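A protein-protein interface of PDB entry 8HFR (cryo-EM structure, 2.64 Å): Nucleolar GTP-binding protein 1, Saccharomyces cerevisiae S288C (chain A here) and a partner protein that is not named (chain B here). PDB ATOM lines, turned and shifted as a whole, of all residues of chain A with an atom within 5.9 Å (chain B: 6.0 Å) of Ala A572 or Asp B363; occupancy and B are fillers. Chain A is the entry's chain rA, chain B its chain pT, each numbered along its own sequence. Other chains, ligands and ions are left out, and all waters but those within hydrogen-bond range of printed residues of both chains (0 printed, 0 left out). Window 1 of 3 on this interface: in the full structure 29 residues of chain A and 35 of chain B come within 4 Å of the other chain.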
ATOM      1  N   PHE A 567      17.863 -24.262  19.866  1.00  0.00           N
ATOM      2  CA  PHE A 567      18.216 -22.862  20.032  1.00  0.00           C
ATOM      3  C   PHE A 567      19.711 -22.606  20.099  1.00  0.00           C
ATOM      4  O   PHE A 567      20.111 -21.440  20.169  1.00  0.00           O
ATOM      5  CB  PHE A 567      17.558 -22.292  21.295  1.00  0.00           C
ATOM      6  CG  PHE A 567      16.227 -21.665  21.045  1.00  0.00           C
ATOM      7  CD1 PHE A 567      16.131 -20.466  20.370  1.00  0.00           C
ATOM      8  CD2 PHE A 567      15.067 -22.277  21.480  1.00  0.00           C
ATOM      9  CE1 PHE A 567      14.906 -19.894  20.134  1.00  0.00           C
ATOM     10  CE2 PHE A 567      13.841 -21.712  21.243  1.00  0.00           C
ATOM     11  CZ  PHE A 567      13.759 -20.520  20.572  1.00  0.00           C
ATOM     12  N   GLN A 570      21.679 -19.818  17.430  1.00  0.00           N
ATOM     13  CA  GLN A 570      20.504 -19.037  17.076  1.00  0.00           C
ATOM     14  C   GLN A 570      20.597 -17.679  17.750  1.00  0.00           C
ATOM     15  O   GLN A 570      21.028 -17.583  18.901  1.00  0.00           O
ATOM     16  CB  GLN A 570      19.204 -19.730  17.503  1.00  0.00           C
ATOM     17  CG  GLN A 570      18.793 -20.936  16.673  1.00  0.00           C
ATOM     18  CD  GLN A 570      18.041 -20.552  15.427  1.00  0.00           C
ATOM     19  OE1 GLN A 570      17.447 -19.480  15.357  1.00  0.00           O
ATOM     20  NE2 GLN A 570      18.042 -21.434  14.436  1.00  0.00           N
ATOM     21  N   ASP A 571      20.199 -16.636  17.030  1.00  0.00           N
ATOM     22  CA  ASP A 571      20.096 -15.301  17.591  1.00  0.00           C
ATOM     23  C   ASP A 571      18.740 -15.138  18.275  1.00  0.00           C
ATOM     24  O   ASP A 571      17.922 -16.061  18.320  1.00  0.00           O
ATOM     25  CB  ASP A 571      20.291 -14.258  16.497  1.00  0.00           C
ATOM     26  CG  ASP A 571      19.494 -14.574  15.238  1.00  0.00           C
ATOM     27  OD1 ASP A 571      18.782 -15.602  15.212  1.00  0.00           O
ATOM     28  OD2 ASP A 571      19.576 -13.793  14.267  1.00  0.00           O
ATOM     29  N   ALA A 572      18.489 -13.950  18.813  1.00  0.00           N
ATOM     30  CA  ALA A 572      17.171 -13.655  19.350  1.00  0.00           C
ATOM     31  C   ALA A 572      16.169 -13.493  18.215  1.00  0.00           C
ATOM     32  O   ALA A 572      16.494 -12.995  17.137  1.00  0.00           O
ATOM     33  CB  ALA A 572      17.208 -12.392  20.200  1.00  0.00           C
ATOM     34  N   LEU A 573      14.941 -13.930  18.463  1.00  0.00           N
ATOM     35  CA  LEU A 573      13.896 -13.888  17.451  1.00  0.00           C
ATOM     36  C   LEU A 573      13.095 -12.596  17.475  1.00  0.00           C
ATOM     37  O   LEU A 573      12.003 -12.554  16.906  1.00  0.00           O
ATOM     38  CB  LEU A 573      12.965 -15.093  17.603  1.00  0.00           C
ATOM     39  CG  LEU A 573      12.349 -15.484  18.947  1.00  0.00           C
ATOM     40  CD1 LEU A 573      11.020 -14.807  19.208  1.00  0.00           C
ATOM     41  CD2 LEU A 573      12.174 -16.985  18.986  1.00  0.00           C
ATOM     42  N   THR A 574      13.602 -11.551  18.114  1.00  0.00           N
ATOM     43  CA  THR A 574      12.930 -10.265  18.170  1.00  0.00           C
ATOM     44  C   THR A 574      13.703  -9.231  17.361  1.00  0.00           C
ATOM     45  O   THR A 574      14.826  -9.467  16.909  1.00  0.00           O
ATOM     46  CB  THR A 574      12.766  -9.794  19.620  1.00  0.00           C
ATOM     47  OG1 THR A 574      14.028  -9.337  20.123  1.00  0.00           O
ATOM     48  CG2 THR A 574      12.258 -10.923  20.490  1.00  0.00           C
ATOM     49  N   VAL B 361       5.607 -18.429  23.942  1.00  0.00           N
ATOM     50  CA  VAL B 361       6.800 -19.096  23.423  1.00  0.00           C
ATOM     51  C   VAL B 361       8.036 -18.464  24.052  1.00  0.00           C
ATOM     52  O   VAL B 361       8.253 -17.258  23.913  1.00  0.00           O
ATOM     53  CB  VAL B 361       6.894 -19.003  21.885  1.00  0.00           C
ATOM     54  CG1 VAL B 361       8.205 -19.577  21.395  1.00  0.00           C
ATOM     55  CG2 VAL B 361       5.743 -19.710  21.209  1.00  0.00           C
ATOM     56  N   ARG B 362       8.859 -19.279  24.705  1.00  0.00           N
ATOM     57  CA  ARG B 362      10.106 -18.833  25.320  1.00  0.00           C
ATOM     58  C   ARG B 362      11.199 -18.657  24.272  1.00  0.00           C
ATOM     59  O   ARG B 362      11.417 -19.540  23.440  1.00  0.00           O
ATOM     60  CB  ARG B 362      10.555 -19.849  26.365  1.00  0.00           C
ATOM     61  CG  ARG B 362      11.931 -19.625  26.943  1.00  0.00           C
ATOM     62  CD  ARG B 362      11.911 -18.674  28.103  1.00  0.00           C
ATOM     63  NE  ARG B 362      13.233 -18.535  28.694  1.00  0.00           N
ATOM     64  CZ  ARG B 362      14.070 -17.543  28.420  1.00  0.00           C
ATOM     65  NH1 ARG B 362      13.716 -16.592  27.573  1.00  0.00           N
ATOM     66  NH2 ARG B 362      15.258 -17.492  29.003  1.00  0.00           N
ATOM     67  N   ASP B 363      11.897 -17.527  24.324  1.00  0.00           N
ATOM     68  CA  ASP B 363      13.041 -17.259  23.455  1.00  0.00           C
ATOM     69  C   ASP B 363      14.305 -17.560  24.252  1.00  0.00           C
ATOM     70  O   ASP B 363      14.721 -16.768  25.097  1.00  0.00           O
ATOM     71  CB  ASP B 363      13.014 -15.818  22.959  1.00  0.00           C
ATOM     72  CG  ASP B 363      14.169 -15.487  22.040  1.00  0.00           C
ATOM     73  OD1 ASP B 363      14.731 -16.402  21.411  1.00  0.00           O
ATOM     74  OD2 ASP B 363      14.508 -14.293  21.935  1.00  0.00           O
ATOM     75  N   PHE B 364      14.920 -18.706  23.974  1.00  0.00           N
ATOM     76  CA  PHE B 364      16.049 -19.175  24.765  1.00  0.00           C
ATOM     77  C   PHE B 364      17.363 -18.497  24.408  1.00  0.00           C
ATOM     78  O   PHE B 364      18.337 -18.652  25.145  1.00  0.00           O
ATOM     79  CB  PHE B 364      16.199 -20.686  24.616  1.00  0.00           C
ATOM     80  CG  PHE B 364      15.409 -21.473  25.613  1.00  0.00           C
ATOM     81  CD1 PHE B 364      15.861 -21.620  26.910  1.00  0.00           C
ATOM     82  CD2 PHE B 364      14.217 -22.074  25.252  1.00  0.00           C
ATOM     83  CE1 PHE B 364      15.136 -22.348  27.832  1.00  0.00           C
ATOM     84  CE2 PHE B 364      13.489 -22.807  26.166  1.00  0.00           C
ATOM     85  CZ  PHE B 364      13.947 -22.943  27.456  1.00  0.00           C
ATOM     86  N   ALA B 365      17.418 -17.753  23.309  1.00  0.00           N
ATOM     87  CA  ALA B 365      18.614 -17.000  22.961  1.00  0.00           C
ATOM     88  C   ALA B 365      18.660 -15.621  23.603  1.00  0.00           C
ATOM     89  O   ALA B 365      19.591 -14.862  23.326  1.00  0.00           O
ATOM     90  CB  ALA B 365      18.722 -16.857  21.446  1.00  0.00           C
ATOM     91  N   GLN B 366      17.687 -15.282  24.438  1.00  0.00           N
ATOM     92  CA  GLN B 366      17.645 -14.024  25.162  1.00  0.00           C
ATOM     93  C   GLN B 366      17.802 -14.291  26.655  1.00  0.00           C
ATOM     94  O   GLN B 366      17.333 -15.308  27.169  1.00  0.00           O
ATOM     95  CB  GLN B 366      16.324 -13.295  24.896  1.00  0.00           C
ATOM     96  CG  GLN B 366      16.295 -11.840  25.318  1.00  0.00           C
ATOM     97  CD  GLN B 366      16.888 -10.928  24.278  1.00  0.00           C
ATOM     98  OE1 GLN B 366      16.488 -10.955  23.122  1.00  0.00           O
ATOM     99  NE2 GLN B 366      17.862 -10.125  24.678  1.00  0.00           N
ATOM    100  N   THR B 367      18.474 -13.375  27.350  1.00  0.00           N
ATOM    101  CA  THR B 367      18.619 -13.472  28.796  1.00  0.00           C
ATOM    102  C   THR B 367      18.703 -12.079  29.411  1.00  0.00           C
ATOM    103  O   THR B 367      19.339 -11.180  28.857  1.00  0.00           O
ATOM    104  CB  THR B 367      19.838 -14.334  29.175  1.00  0.00           C
ATOM    105  OG1 THR B 367      19.999 -14.355  30.600  1.00  0.00           O
ATOM    106  CG2 THR B 367      21.115 -13.860  28.493  1.00  0.00           C
ATOM    107  N   TYR B 430      11.411  -9.133  26.489  1.00  0.00           N
ATOM    108  CA  TYR B 430      11.524 -10.005  25.323  1.00  0.00           C
ATOM    109  C   TYR B 430      11.993 -11.407  25.665  1.00  0.00           C
ATOM    110  O   TYR B 430      12.528 -12.102  24.805  1.00  0.00           O
ATOM    111  CB  TYR B 430      12.437  -9.409  24.249  1.00  0.00           C
ATOM    112  CG  TYR B 430      12.075  -8.013  23.834  1.00  0.00           C
ATOM    113  CD1 TYR B 430      10.926  -7.765  23.103  1.00  0.00           C
ATOM    114  CD2 TYR B 430      12.883  -6.942  24.170  1.00  0.00           C
ATOM    115  CE1 TYR B 430      10.593  -6.493  22.716  1.00  0.00           C
ATOM    116  CE2 TYR B 430      12.555  -5.661  23.789  1.00  0.00           C
ATOM    117  CZ  TYR B 430      11.409  -5.446  23.060  1.00  0.00           C
ATOM    118  OH  TYR B 430      11.081  -4.174  22.675  1.00  0.00           O
ATOM    119  N   LEU B 431      11.787 -11.856  26.900  1.00  0.00           N
ATOM    120  CA  LEU B 431      12.170 -13.215  27.248  1.00  0.00           C
ATOM    121  C   LEU B 431      11.168 -14.235  26.738  1.00  0.00           C
ATOM    122  O   LEU B 431      11.480 -15.426  26.710  1.00  0.00           O
ATOM    123  CB  LEU B 431      12.317 -13.354  28.760  1.00  0.00           C
ATOM    124  CG  LEU B 431      13.413 -12.580  29.490  1.00  0.00           C
ATOM    125  CD1 LEU B 431      13.617 -13.155  30.866  1.00  0.00           C
ATOM    126  CD2 LEU B 431      14.704 -12.609  28.725  1.00  0.00           C
ATOM    127  N   CYS B 432       9.985 -13.796  26.323  1.00  0.00           N
ATOM    128  CA  CYS B 432       8.917 -14.695  25.927  1.00  0.00           C
ATOM    129  C   CYS B 432       7.958 -13.925  25.036  1.00  0.00           C
ATOM    130  O   CYS B 432       7.739 -12.732  25.245  1.00  0.00           O
ATOM    131  CB  CYS B 432       8.205 -15.250  27.162  1.00  0.00           C
ATOM    132  SG  CYS B 432       7.041 -16.573  26.865  1.00  0.00           S
ATOM    133  N   VAL B 433       7.401 -14.604  24.032  1.00  0.00           N
ATOM    134  CA  VAL B 433       6.516 -13.986  23.055  1.00  0.00           C
ATOM    135  C   VAL B 433       5.239 -14.803  22.946  1.00  0.00           C
ATOM    136  O   VAL B 433       5.205 -15.989  23.267  1.00  0.00           O
ATOM    137  CB  VAL B 433       7.171 -13.858  21.669  1.00  0.00           C
ATOM    138  CG1 VAL B 433       8.196 -12.743  21.662  1.00  0.00           C
ATOM    139  CG2 VAL B 433       7.806 -15.164  21.276  1.00  0.00           C
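Arg B362 touches Phe A567.
Asp B363 touches Phe A567.
Phe B364 touches Phe A567 (CB to CD2, 3.7 Å).
Gln A570 touches Ala B365.
Asp A571 touches Ala B365 (O to CB, 3.3 Å).
Asp B363 touches Ala A572 (OD2 to CB, 3.7 Å).
Ala B365 touches Ala A572.
CB of Ala A572 touches OE1 of Gln B366, 3.3 Å away.
Leu A573 touches Asp B363 (N to OD2, 3.5 Å).
Val B433 touches Leu A573 (CG2 to CD1, 3.8 Å).
Printed residues of chain B that touch a printed residue of chain A: Arg B362, Asp B363, Phe B364, Ala B365, Gln B366 and Val B433.
Hydrophobic or aromatic side chains of chain B that line the printed part of chain A: Phe B364, Ala B365 and Val B433.
Of the 6 printed residues of chain A, 5 touch a printed residue of chain B.
Hydrophobic or aromatic side chains of chain A within 4 Å of the printed part of chain B: Phe A567, Ala A572 and Leu A573.
Among the printed residues, no Asp or Glu carboxylate lies within 4 Å of a Lys or Arg side-chain nitrogen of the other chain.
Printed residues of chain B within 4 Å of Phe A567: Arg B362, Asp B363 and Phe B364.
Of the printed residues of chain B, Asp A571 touches Ala B365.
Ala A572 touches just these residues of chain B: Asp B363 (3.7 Å), Ala B365 (3.9 Å) and Gln B366 (3.3 Å).
Asp B363 touches just these residues of chain A: Phe A567 (3.7 Å), Ala A572 (3.7 Å) and Leu A573 (3.5 Å).
Printed residues of chain A within 4 Å of Gln B366: Ala A572 (3.3 Å).
Tyr B430 touches none of the printed residues of chain A.
Leu B431 touches none of the printed residues of chain A.
The nearest printed residue of chain B that does not touch Ala A572 is Tyr B430 (6.6 Å).
The nearest printed residue of chain A that does not touch Gln B366 is Thr A574 (4.2 Å).
The backbone NH of Val B361 sits at hydrogen-bond distance from the backbone carbonyl oxygen of Val B433 (2.6 Å).
O of Leu B431 sits at hydrogen-bond distance from NH1 of Arg B362 (2.7 Å).
N of Asp B363 lies within hydrogen-bond range of O of Leu B431, at 3.2 Å.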
